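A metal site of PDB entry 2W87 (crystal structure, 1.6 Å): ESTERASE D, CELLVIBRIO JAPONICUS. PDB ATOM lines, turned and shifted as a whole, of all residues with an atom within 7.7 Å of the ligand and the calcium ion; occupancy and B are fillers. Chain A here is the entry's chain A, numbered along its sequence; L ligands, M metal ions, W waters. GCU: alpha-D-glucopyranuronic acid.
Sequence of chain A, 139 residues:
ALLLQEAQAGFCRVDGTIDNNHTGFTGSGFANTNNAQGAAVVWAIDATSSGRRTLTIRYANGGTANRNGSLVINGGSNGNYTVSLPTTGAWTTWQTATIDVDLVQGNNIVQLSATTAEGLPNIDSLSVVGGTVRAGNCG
ND2 of Asn 122 sits at hydrogen-bond distance from O3 of the ligand (2.9 Å). The guanidinium group (NH2) of Arg 67 lies within salt-bridge range of an oxygen (O6B) of the ligand, at 2.8 Å. A ring nitrogen (NE2) of His 22 is in hydrogen-bond range of an oxygen (O2) of the ligand (2.8 Å).
The side-chain amide nitrogen (ND2) of Asn 32 is in hydrogen-bond range of the side-chain carboxylate (OD2) of Asp 19, at 2.8 Å. The side-chain amide oxygen (OD1) of Asn 32 sits close to the side-chain amide oxygen (OD1) of Asn 122. The side-chain amide oxygen (OD1) of Asn 35 sits close to the backbone carbonyl oxygen (O) of Glu 118 (3.4 Å). O of Thr 17 sits at hydrogen-bond distance from N of Asn 32, at 2.8 Å. The backbone carbonyl oxygen (O) of Asn 122 lies within hydrogen-bond range of the backbone NH (N) of Ala 60. The guanidinium group (NH2) of Arg 67 lies within salt-bridge range of the side-chain carboxylate (OE1) of Glu 118 (3.0 Å). The backbone carbonyl oxygen (O) of Leu 120 sits at hydrogen-bond distance from the guanidinium group (NH1) of Arg 67 (3.1 Å). The side-chain hydroxyl of Thr 33 sits at hydrogen-bond distance from the backbone NH of Leu 120, at 2.8 Å.
Trp 91 touches the ligand. Hydrophobic or aromatic side chains within 4 Å of the ligand: His 22 and Trp 91. Six residues have an atom within 4 Å of the ligand: His 22, Asn 32, Asn 35, Arg 67, Trp 91 and Asn 122.
The nearest printed residue that does not touch the calcium ion is Asn 122 (4.3 Å).
The calcium ion is bound by OD1 of Asn 32 (2.3 Å), O of Thr 33 (2.4 Å), O6A of the ligand (2.4 Å), water W5 (2.4 Å), water W3 (2.5 Å), water W2 (2.5 Å), OD1 of Asn 35 (2.6 Å) and O4 of the ligand (2.7 Å). The calcium ion has eight donor atoms within binding distance.
Water W3 lies within hydrogen-bond range of the backbone carbonyl oxygen of Glu 118, the backbone carbonyl oxygen of Leu 120, the side-chain hydroxyl of Thr 33 and the guanidinium group of Arg 67. Water W4 lies within hydrogen-bond range of the side-chain amide oxygen (OD1) of Asn 21 (2.7 Å), an oxygen (O3) of the ligand (2.7 Å), the side-chain carboxylate (OD2) of Asp 19 (2.7 Å) and the side-chain amide nitrogen (ND2) of Asn 32 (3.4 Å). Water W7 lies within hydrogen-bond range of an oxygen (O2) of the ligand (2.8 Å) and the side-chain amide nitrogen of Asn 21 (3.3 Å). Water W6 lies within hydrogen-bond range of the side-chain amide nitrogen of Asn 32 and an oxygen (O1) of the ligand.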
ATOM      1  N   ASP A  15      25.215 -20.329   1.658  1.00  0.00           N
ATOM      2  CA  ASP A  15      25.600 -20.212   3.053  1.00  0.00           C
ATOM      3  C   ASP A  15      25.382 -21.568   3.691  1.00  0.00           C
ATOM      4  O   ASP A  15      24.302 -21.866   4.199  1.00  0.00           O
ATOM      5  CB  ASP A  15      24.770 -19.148   3.751  1.00  0.00           C
ATOM      6  CG  ASP A  15      24.923 -17.789   3.116  1.00  0.00           C
ATOM      7  OD1 ASP A  15      26.105 -17.441   2.782  1.00  0.00           O
ATOM      8  OD2 ASP A  15      23.877 -17.095   2.902  1.00  0.00           O
ATOM      9  N   GLY A  16      26.416 -22.390   3.622  1.00  0.00           N
ATOM     10  CA  GLY A  16      26.285 -23.819   3.918  1.00  0.00           C
ATOM     11  C   GLY A  16      27.249 -24.609   3.053  1.00  0.00           C
ATOM     12  O   GLY A  16      28.376 -24.193   2.834  1.00  0.00           O
ATOM     13  N   THR A  17      26.810 -25.744   2.516  1.00  0.00           N
ATOM     14  CA  THR A  17      27.668 -26.601   1.719  1.00  0.00           C
ATOM     15  C   THR A  17      26.953 -27.073   0.481  1.00  0.00           C
ATOM     16  O   THR A  17      25.738 -27.013   0.414  1.00  0.00           O
ATOM     17  CB  THR A  17      28.128 -27.855   2.517  1.00  0.00           C
ATOM     18  OG1 THR A  17      27.012 -28.517   3.132  1.00  0.00           O
ATOM     19  CG2 THR A  17      29.152 -27.488   3.579  1.00  0.00           C
ATOM     20  N   ASP A  19      26.315 -30.579  -1.165  1.00  0.00           N
ATOM     21  CA  ASP A  19      26.317 -31.941  -0.675  1.00  0.00           C
ATOM     22  C   ASP A  19      25.763 -32.873  -1.741  1.00  0.00           C
ATOM     23  O   ASP A  19      25.163 -32.441  -2.745  1.00  0.00           O
ATOM     24  CB  ASP A  19      25.441 -32.075   0.577  1.00  0.00           C
ATOM     25  CG  ASP A  19      25.969 -31.340   1.769  1.00  0.00           C
ATOM     26  OD1 ASP A  19      27.033 -30.688   1.690  1.00  0.00           O
ATOM     27  OD2 ASP A  19      25.303 -31.447   2.821  1.00  0.00           O
ATOM     28  N   ASN A  21      24.897 -36.453  -0.424  1.00  0.00           N
ATOM     29  CA  ASN A  21      24.702 -37.650   0.415  1.00  0.00           C
ATOM     30  C   ASN A  21      23.243 -38.108   0.556  1.00  0.00           C
ATOM     31  O   ASN A  21      22.933 -38.935   1.421  1.00  0.00           O
ATOM     32  CB  ASN A  21      25.290 -37.405   1.804  1.00  0.00           C
ATOM     33  CG  ASN A  21      24.575 -36.302   2.559  1.00  0.00           C
ATOM     34  OD1 ASN A  21      24.098 -35.350   1.950  1.00  0.00           O
ATOM     35  ND2 ASN A  21      24.470 -36.430   3.874  1.00  0.00           N
ATOM     36  N   HIS A  22      22.356 -37.551  -0.249  1.00  0.00           N
ATOM     37  CA  HIS A  22      21.003 -38.071  -0.381  1.00  0.00           C
ATOM     38  C   HIS A  22      20.732 -38.239  -1.858  1.00  0.00           C
ATOM     39  O   HIS A  22      21.020 -37.343  -2.632  1.00  0.00           O
ATOM     40  CB  HIS A  22      19.974 -37.077   0.173  1.00  0.00           C
ATOM     41  CG  HIS A  22      20.136 -36.762   1.624  1.00  0.00           C
ATOM     42  ND1 HIS A  22      20.010 -37.725   2.608  1.00  0.00           N
ATOM     43  CD2 HIS A  22      20.359 -35.592   2.264  1.00  0.00           C
ATOM     44  CE1 HIS A  22      20.171 -37.148   3.786  1.00  0.00           C
ATOM     45  NE2 HIS A  22      20.396 -35.864   3.606  1.00  0.00           N
ATOM     46  N   PHE A  30      23.520 -30.852  -4.411  1.00  0.00           N
ATOM     47  CA  PHE A  30      22.475 -29.916  -4.009  1.00  0.00           C
ATOM     48  C   PHE A  30      23.049 -28.964  -2.977  1.00  0.00           C
ATOM     49  O   PHE A  30      24.042 -29.266  -2.325  1.00  0.00           O
ATOM     50  CB  PHE A  30      21.277 -30.671  -3.443  1.00  0.00           C
ATOM     51  CG  PHE A  30      21.617 -31.665  -2.363  1.00  0.00           C
ATOM     52  CD1 PHE A  30      21.729 -31.265  -1.040  1.00  0.00           C
ATOM     53  CD2 PHE A  30      21.794 -33.005  -2.654  1.00  0.00           C
ATOM     54  CE1 PHE A  30      22.025 -32.168  -0.052  1.00  0.00           C
ATOM     55  CE2 PHE A  30      22.079 -33.916  -1.665  1.00  0.00           C
ATOM     56  CZ  PHE A  30      22.194 -33.509  -0.363  1.00  0.00           C
ATOM     57  N   ALA A  31      22.453 -27.781  -2.893  1.00  0.00           N
ATOM     58  CA  ALA A  31      22.896 -26.786  -1.918  1.00  0.00           C
ATOM     59  C   ALA A  31      22.185 -27.081  -0.585  1.00  0.00           C
ATOM     60  O   ALA A  31      20.950 -27.155  -0.522  1.00  0.00           O
ATOM     61  CB  ALA A  31      22.570 -25.377  -2.409  1.00  0.00           C
ATOM     62  N   ASN A  32      22.987 -27.188   0.475  1.00  0.00           N
ATOM     63  CA  ASN A  32      22.490 -27.439   1.815  1.00  0.00           C
ATOM     64  C   ASN A  32      22.797 -26.239   2.720  1.00  0.00           C
ATOM     65  O   ASN A  32      23.934 -26.068   3.145  1.00  0.00           O
ATOM     66  CB  ASN A  32      23.174 -28.686   2.373  1.00  0.00           C
ATOM     67  CG  ASN A  32      22.821 -28.960   3.822  1.00  0.00           C
ATOM     68  OD1 ASN A  32      22.015 -28.243   4.435  1.00  0.00           O
ATOM     69  ND2 ASN A  32      23.449 -30.012   4.393  1.00  0.00           N
ATOM     70  N   THR A  33      21.815 -25.395   2.980  1.00  0.00           N
ATOM     71  CA  THR A  33      22.040 -24.217   3.824  1.00  0.00           C
ATOM     72  C   THR A  33      22.305 -24.602   5.281  1.00  0.00           C
ATOM     73  O   THR A  33      21.763 -25.595   5.789  1.00  0.00           O
ATOM     74  CB  THR A  33      20.833 -23.246   3.847  1.00  0.00           C
ATOM     75  OG1 THR A  33      19.653 -23.925   4.266  1.00  0.00           O
ATOM     76  CG2 THR A  33      20.634 -22.612   2.474  1.00  0.00           C
ATOM     77  N   ASN A  34      23.148 -23.807   5.928  1.00  0.00           N
ATOM     78  CA  ASN A  34      23.155 -23.700   7.361  1.00  0.00           C
ATOM     79  C   ASN A  34      21.737 -23.671   7.892  1.00  0.00           C
ATOM     80  O   ASN A  34      20.860 -23.095   7.257  1.00  0.00           O
ATOM     81  CB  ASN A  34      23.798 -22.370   7.783  1.00  0.00           C
ATOM     82  CG  ASN A  34      25.290 -22.288   7.455  1.00  0.00           C
ATOM     83  OD1 ASN A  34      25.978 -23.306   7.427  1.00  0.00           O
ATOM     84  ND2 ASN A  34      25.802 -21.061   7.239  1.00  0.00           N
ATOM     85  N   ASN A  35      21.517 -24.246   9.069  1.00  0.00           N
ATOM     86  CA  ASN A  35      20.216 -24.202   9.714  1.00  0.00           C
ATOM     87  C   ASN A  35      20.093 -22.922  10.545  1.00  0.00           C
ATOM     88  O   ASN A  35      20.265 -22.930  11.774  1.00  0.00           O
ATOM     89  CB  ASN A  35      20.015 -25.476  10.528  1.00  0.00           C
ATOM     90  CG  ASN A  35      20.347 -26.729   9.722  1.00  0.00           C
ATOM     91  OD1 ASN A  35      20.121 -26.767   8.503  1.00  0.00           O
ATOM     92  ND2 ASN A  35      20.939 -27.715  10.374  1.00  0.00           N
ATOM     93  N   ALA A  36      19.819 -21.833   9.852  1.00  0.00           N
ATOM     94  CA  ALA A  36      19.715 -20.507  10.415  1.00  0.00           C
ATOM     95  C   ALA A  36      18.821 -19.658   9.543  1.00  0.00           C
ATOM     96  O   ALA A  36      18.825 -19.771   8.315  1.00  0.00           O
ATOM     97  CB  ALA A  36      21.088 -19.875  10.499  1.00  0.00           C
ATOM     98  N   ALA A  39      19.890 -17.857   5.981  1.00  0.00           N
ATOM     99  CA  ALA A  39      20.836 -18.620   5.171  1.00  0.00           C
ATOM    100  C   ALA A  39      20.311 -18.750   3.731  1.00  0.00           C
ATOM    101  O   ALA A  39      19.142 -19.082   3.512  1.00  0.00           O
ATOM    102  CB  ALA A  39      21.116 -19.982   5.799  1.00  0.00           C
ATOM    103  N   ALA A  60      14.323 -30.713  -1.659  1.00  0.00           N
ATOM    104  CA  ALA A  60      13.920 -31.793  -0.764  1.00  0.00           C
ATOM    105  C   ALA A  60      13.837 -31.231   0.633  1.00  0.00           C
ATOM    106  O   ALA A  60      14.710 -30.501   1.035  1.00  0.00           O
ATOM    107  CB  ALA A  60      14.935 -32.921  -0.799  1.00  0.00           C
ATOM    108  N   ASN A  61      12.784 -31.580   1.365  1.00  0.00           N
ATOM    109  CA  ASN A  61      12.589 -31.096   2.721  1.00  0.00           C
ATOM    110  C   ASN A  61      12.142 -32.285   3.557  1.00  0.00           C
ATOM    111  O   ASN A  61      10.967 -32.598   3.574  1.00  0.00           O
ATOM    112  CB  ASN A  61      11.560 -29.972   2.748  1.00  0.00           C
ATOM    113  CG  ASN A  61      11.314 -29.430   4.129  1.00  0.00           C
ATOM    114  OD1 ASN A  61      11.851 -29.931   5.124  1.00  0.00           O
ATOM    115  ND2 ASN A  61      10.477 -28.397   4.212  1.00  0.00           N
ATOM    116  N   GLY A  62      13.094 -32.925   4.224  1.00  0.00           N
ATOM    117  CA  GLY A  62      12.829 -34.087   5.072  1.00  0.00           C
ATOM    118  C   GLY A  62      12.568 -33.688   6.519  1.00  0.00           C
ATOM    119  O   GLY A  62      12.512 -34.534   7.415  1.00  0.00           O
ATOM    120  N   GLY A  63      12.415 -32.384   6.747  1.00  0.00           N
ATOM    121  CA  GLY A  63      12.092 -31.882   8.080  1.00  0.00           C
ATOM    122  C   GLY A  63      10.607 -32.002   8.304  1.00  0.00           C
ATOM    123  O   GLY A  63       9.898 -32.524   7.441  1.00  0.00           O
ATOM    124  N   ARG A  67       9.813 -24.824   5.213  1.00  0.00           N
ATOM    125  CA  ARG A  67      11.005 -24.015   5.327  1.00  0.00           C
ATOM    126  C   ARG A  67      10.931 -22.956   4.220  1.00  0.00           C
ATOM    127  O   ARG A  67      11.762 -22.935   3.285  1.00  0.00           O
ATOM    128  CB  ARG A  67      12.208 -24.904   5.181  1.00  0.00           C
ATOM    129  CG  ARG A  67      12.392 -25.852   6.298  1.00  0.00           C
ATOM    130  CD  ARG A  67      13.704 -26.554   6.142  1.00  0.00           C
ATOM    131  NE  ARG A  67      13.917 -27.557   7.185  1.00  0.00           N
ATOM    132  CZ  ARG A  67      15.089 -28.135   7.417  1.00  0.00           C
ATOM    133  NH1 ARG A  67      16.151 -27.822   6.688  1.00  0.00           N
ATOM    134  NH2 ARG A  67      15.194 -29.029   8.391  1.00  0.00           N
ATOM    135  N   TRP A  91      14.499 -36.653   2.793  1.00  0.00           N
ATOM    136  CA  TRP A  91      15.580 -35.933   2.138  1.00  0.00           C
ATOM    137  C   TRP A  91      15.908 -36.493   0.750  1.00  0.00           C
ATOM    138  O   TRP A  91      16.662 -35.908  -0.031  1.00  0.00           O
ATOM    139  CB  TRP A  91      16.846 -35.904   3.010  1.00  0.00           C
ATOM    140  CG  TRP A  91      16.647 -35.157   4.260  1.00  0.00           C
ATOM    141  CD1 TRP A  91      16.559 -35.656   5.528  1.00  0.00           C
ATOM    142  CD2 TRP A  91      16.433 -33.740   4.379  1.00  0.00           C
ATOM    143  NE1 TRP A  91      16.336 -34.655   6.428  1.00  0.00           N
ATOM    144  CE2 TRP A  91      16.252 -33.453   5.751  1.00  0.00           C
ATOM    145  CE3 TRP A  91      16.392 -32.679   3.473  1.00  0.00           C
ATOM    146  CZ2 TRP A  91      16.024 -32.166   6.237  1.00  0.00           C
ATOM    147  CZ3 TRP A  91      16.161 -31.388   3.951  1.00  0.00           C
ATOM    148  CH2 TRP A  91      15.986 -31.133   5.316  1.00  0.00           C
ATOM    149  N   GLU A 118      15.331 -23.058  10.725  1.00  0.00           N
ATOM    150  CA  GLU A 118      15.772 -24.350  10.176  1.00  0.00           C
ATOM    151  C   GLU A 118      16.579 -24.184   8.885  1.00  0.00           C
ATOM    152  O   GLU A 118      17.174 -25.134   8.406  1.00  0.00           O
ATOM    153  CB  GLU A 118      14.580 -25.251   9.876  1.00  0.00           C
ATOM    154  CG  GLU A 118      13.804 -25.702  11.086  1.00  0.00           C
ATOM    155  CD  GLU A 118      12.949 -26.929  10.788  1.00  0.00           C
ATOM    156  OE1 GLU A 118      13.518 -28.040  10.678  1.00  0.00           O
ATOM    157  OE2 GLU A 118      11.707 -26.773  10.719  1.00  0.00           O
ATOM    158  N   GLY A 119      16.615 -22.970   8.355  1.00  0.00           N
ATOM    159  CA  GLY A 119      17.281 -22.754   7.084  1.00  0.00           C
ATOM    160  C   GLY A 119      16.346 -23.160   5.955  1.00  0.00           C
ATOM    161  O   GLY A 119      15.127 -23.287   6.140  1.00  0.00           O
ATOM    162  N   LEU A 120      16.908 -23.348   4.764  1.00  0.00           N
ATOM    163  CA  LEU A 120      16.129 -23.789   3.627  1.00  0.00           C
ATOM    164  C   LEU A 120      16.025 -25.309   3.548  1.00  0.00           C
ATOM    165  O   LEU A 120      16.736 -26.027   4.226  1.00  0.00           O
ATOM    166  CB  LEU A 120      16.776 -23.274   2.334  1.00  0.00           C
ATOM    167  CG  LEU A 120      16.674 -21.777   2.068  1.00  0.00           C
ATOM    168  CD1 LEU A 120      17.496 -21.427   0.778  1.00  0.00           C
ATOM    169  CD2 LEU A 120      15.224 -21.344   1.899  1.00  0.00           C
ATOM    170  N   PRO A 121      15.136 -25.802   2.666  1.00  0.00           N
ATOM    171  CA  PRO A 121      15.285 -27.190   2.291  1.00  0.00           C
ATOM    172  C   PRO A 121      16.602 -27.345   1.527  1.00  0.00           C
ATOM    173  O   PRO A 121      17.294 -26.341   1.260  1.00  0.00           O
ATOM    174  CB  PRO A 121      14.116 -27.426   1.351  1.00  0.00           C
ATOM    175  CG  PRO A 121      13.262 -26.276   1.427  1.00  0.00           C
ATOM    176  CD  PRO A 121      14.081 -25.122   1.905  1.00  0.00           C
ATOM    177  N   ASN A 122      16.964 -28.580   1.190  1.00  0.00           N
ATOM    178  CA  ASN A 122      18.081 -28.792   0.275  1.00  0.00           C
ATOM    179  C   ASN A 122      17.629 -28.413  -1.133  1.00  0.00           C
ATOM    180  O   ASN A 122      16.540 -28.816  -1.560  1.00  0.00           O
ATOM    181  CB  ASN A 122      18.520 -30.255   0.329  1.00  0.00           C
ATOM    182  CG  ASN A 122      19.222 -30.621   1.632  1.00  0.00           C
ATOM    183  OD1 ASN A 122      19.770 -29.745   2.342  1.00  0.00           O
ATOM    184  ND2 ASN A 122      19.262 -31.901   1.946  1.00  0.00           N
ATOM    185  N   ILE A 123      18.437 -27.648  -1.847  1.00  0.00           N
ATOM    186  CA  ILE A 123      18.042 -27.091  -3.155  1.00  0.00           C
ATOM    187  C   ILE A 123      18.846 -27.734  -4.264  1.00  0.00           C
ATOM    188  O   ILE A 123      20.055 -27.579  -4.348  1.00  0.00           O
ATOM    189  CB  ILE A 123      18.251 -25.553  -3.216  1.00  0.00           C
ATOM    190  CG1 ILE A 123      17.564 -24.861  -2.024  1.00  0.00           C
ATOM    191  CG2 ILE A 123      17.878 -25.006  -4.597  1.00  0.00           C
ATOM    192  CD1 ILE A 123      16.065 -25.029  -1.949  1.00  0.00           C
HETATM  193  C1  GCU L   1      20.081 -33.397   7.841  1.00  0.00           C
HETATM  194  C2  GCU L   1      20.137 -33.713   6.339  1.00  0.00           C
HETATM  195  C3  GCU L   1      20.669 -32.491   5.592  1.00  0.00           C
HETATM  196  C4  GCU L   1      19.710 -31.345   5.827  1.00  0.00           C
HETATM  197  C5  GCU L   1      19.596 -31.106   7.337  1.00  0.00           C
HETATM  198  C6  GCU L   1      18.604 -30.006   7.680  1.00  0.00           C
HETATM  199  O1  GCU L   1      21.413 -33.076   8.238  1.00  0.00           O
HETATM  200  O2  GCU L   1      21.011 -34.813   6.125  1.00  0.00           O
HETATM  201  O3  GCU L   1      20.794 -32.764   4.190  1.00  0.00           O
HETATM  202  O4  GCU L   1      20.175 -30.121   5.202  1.00  0.00           O
HETATM  203  O5  GCU L   1      19.144 -32.297   7.985  1.00  0.00           O
HETATM  204  O6A GCU L   1      18.723 -28.946   7.042  1.00  0.00           O
HETATM  205  O6B GCU L   1      17.738 -30.207   8.564  1.00  0.00           O
HETATM  206 CA    CA M   1      20.444 -27.574   6.039  1.00  0.00          CA
HETATM  207  O   HOH W   1      17.383 -32.254  10.290  1.00  0.00           O
HETATM  208  O   HOH W   2      19.240 -27.390   3.887  1.00  0.00           O
HETATM  209  O   HOH W   3      18.668 -25.870   6.209  1.00  0.00           O
HETATM  210  O   HOH W   4      23.287 -33.173   3.282  1.00  0.00           O
HETATM  211  O   HOH W   5      22.223 -28.319   7.521  1.00  0.00           O
HETATM  212  O   HOH W   6      23.561 -30.863   7.242  1.00  0.00           O
HETATM  213  O   HOH W   7      23.730 -34.276   6.255  1.00  0.00           O
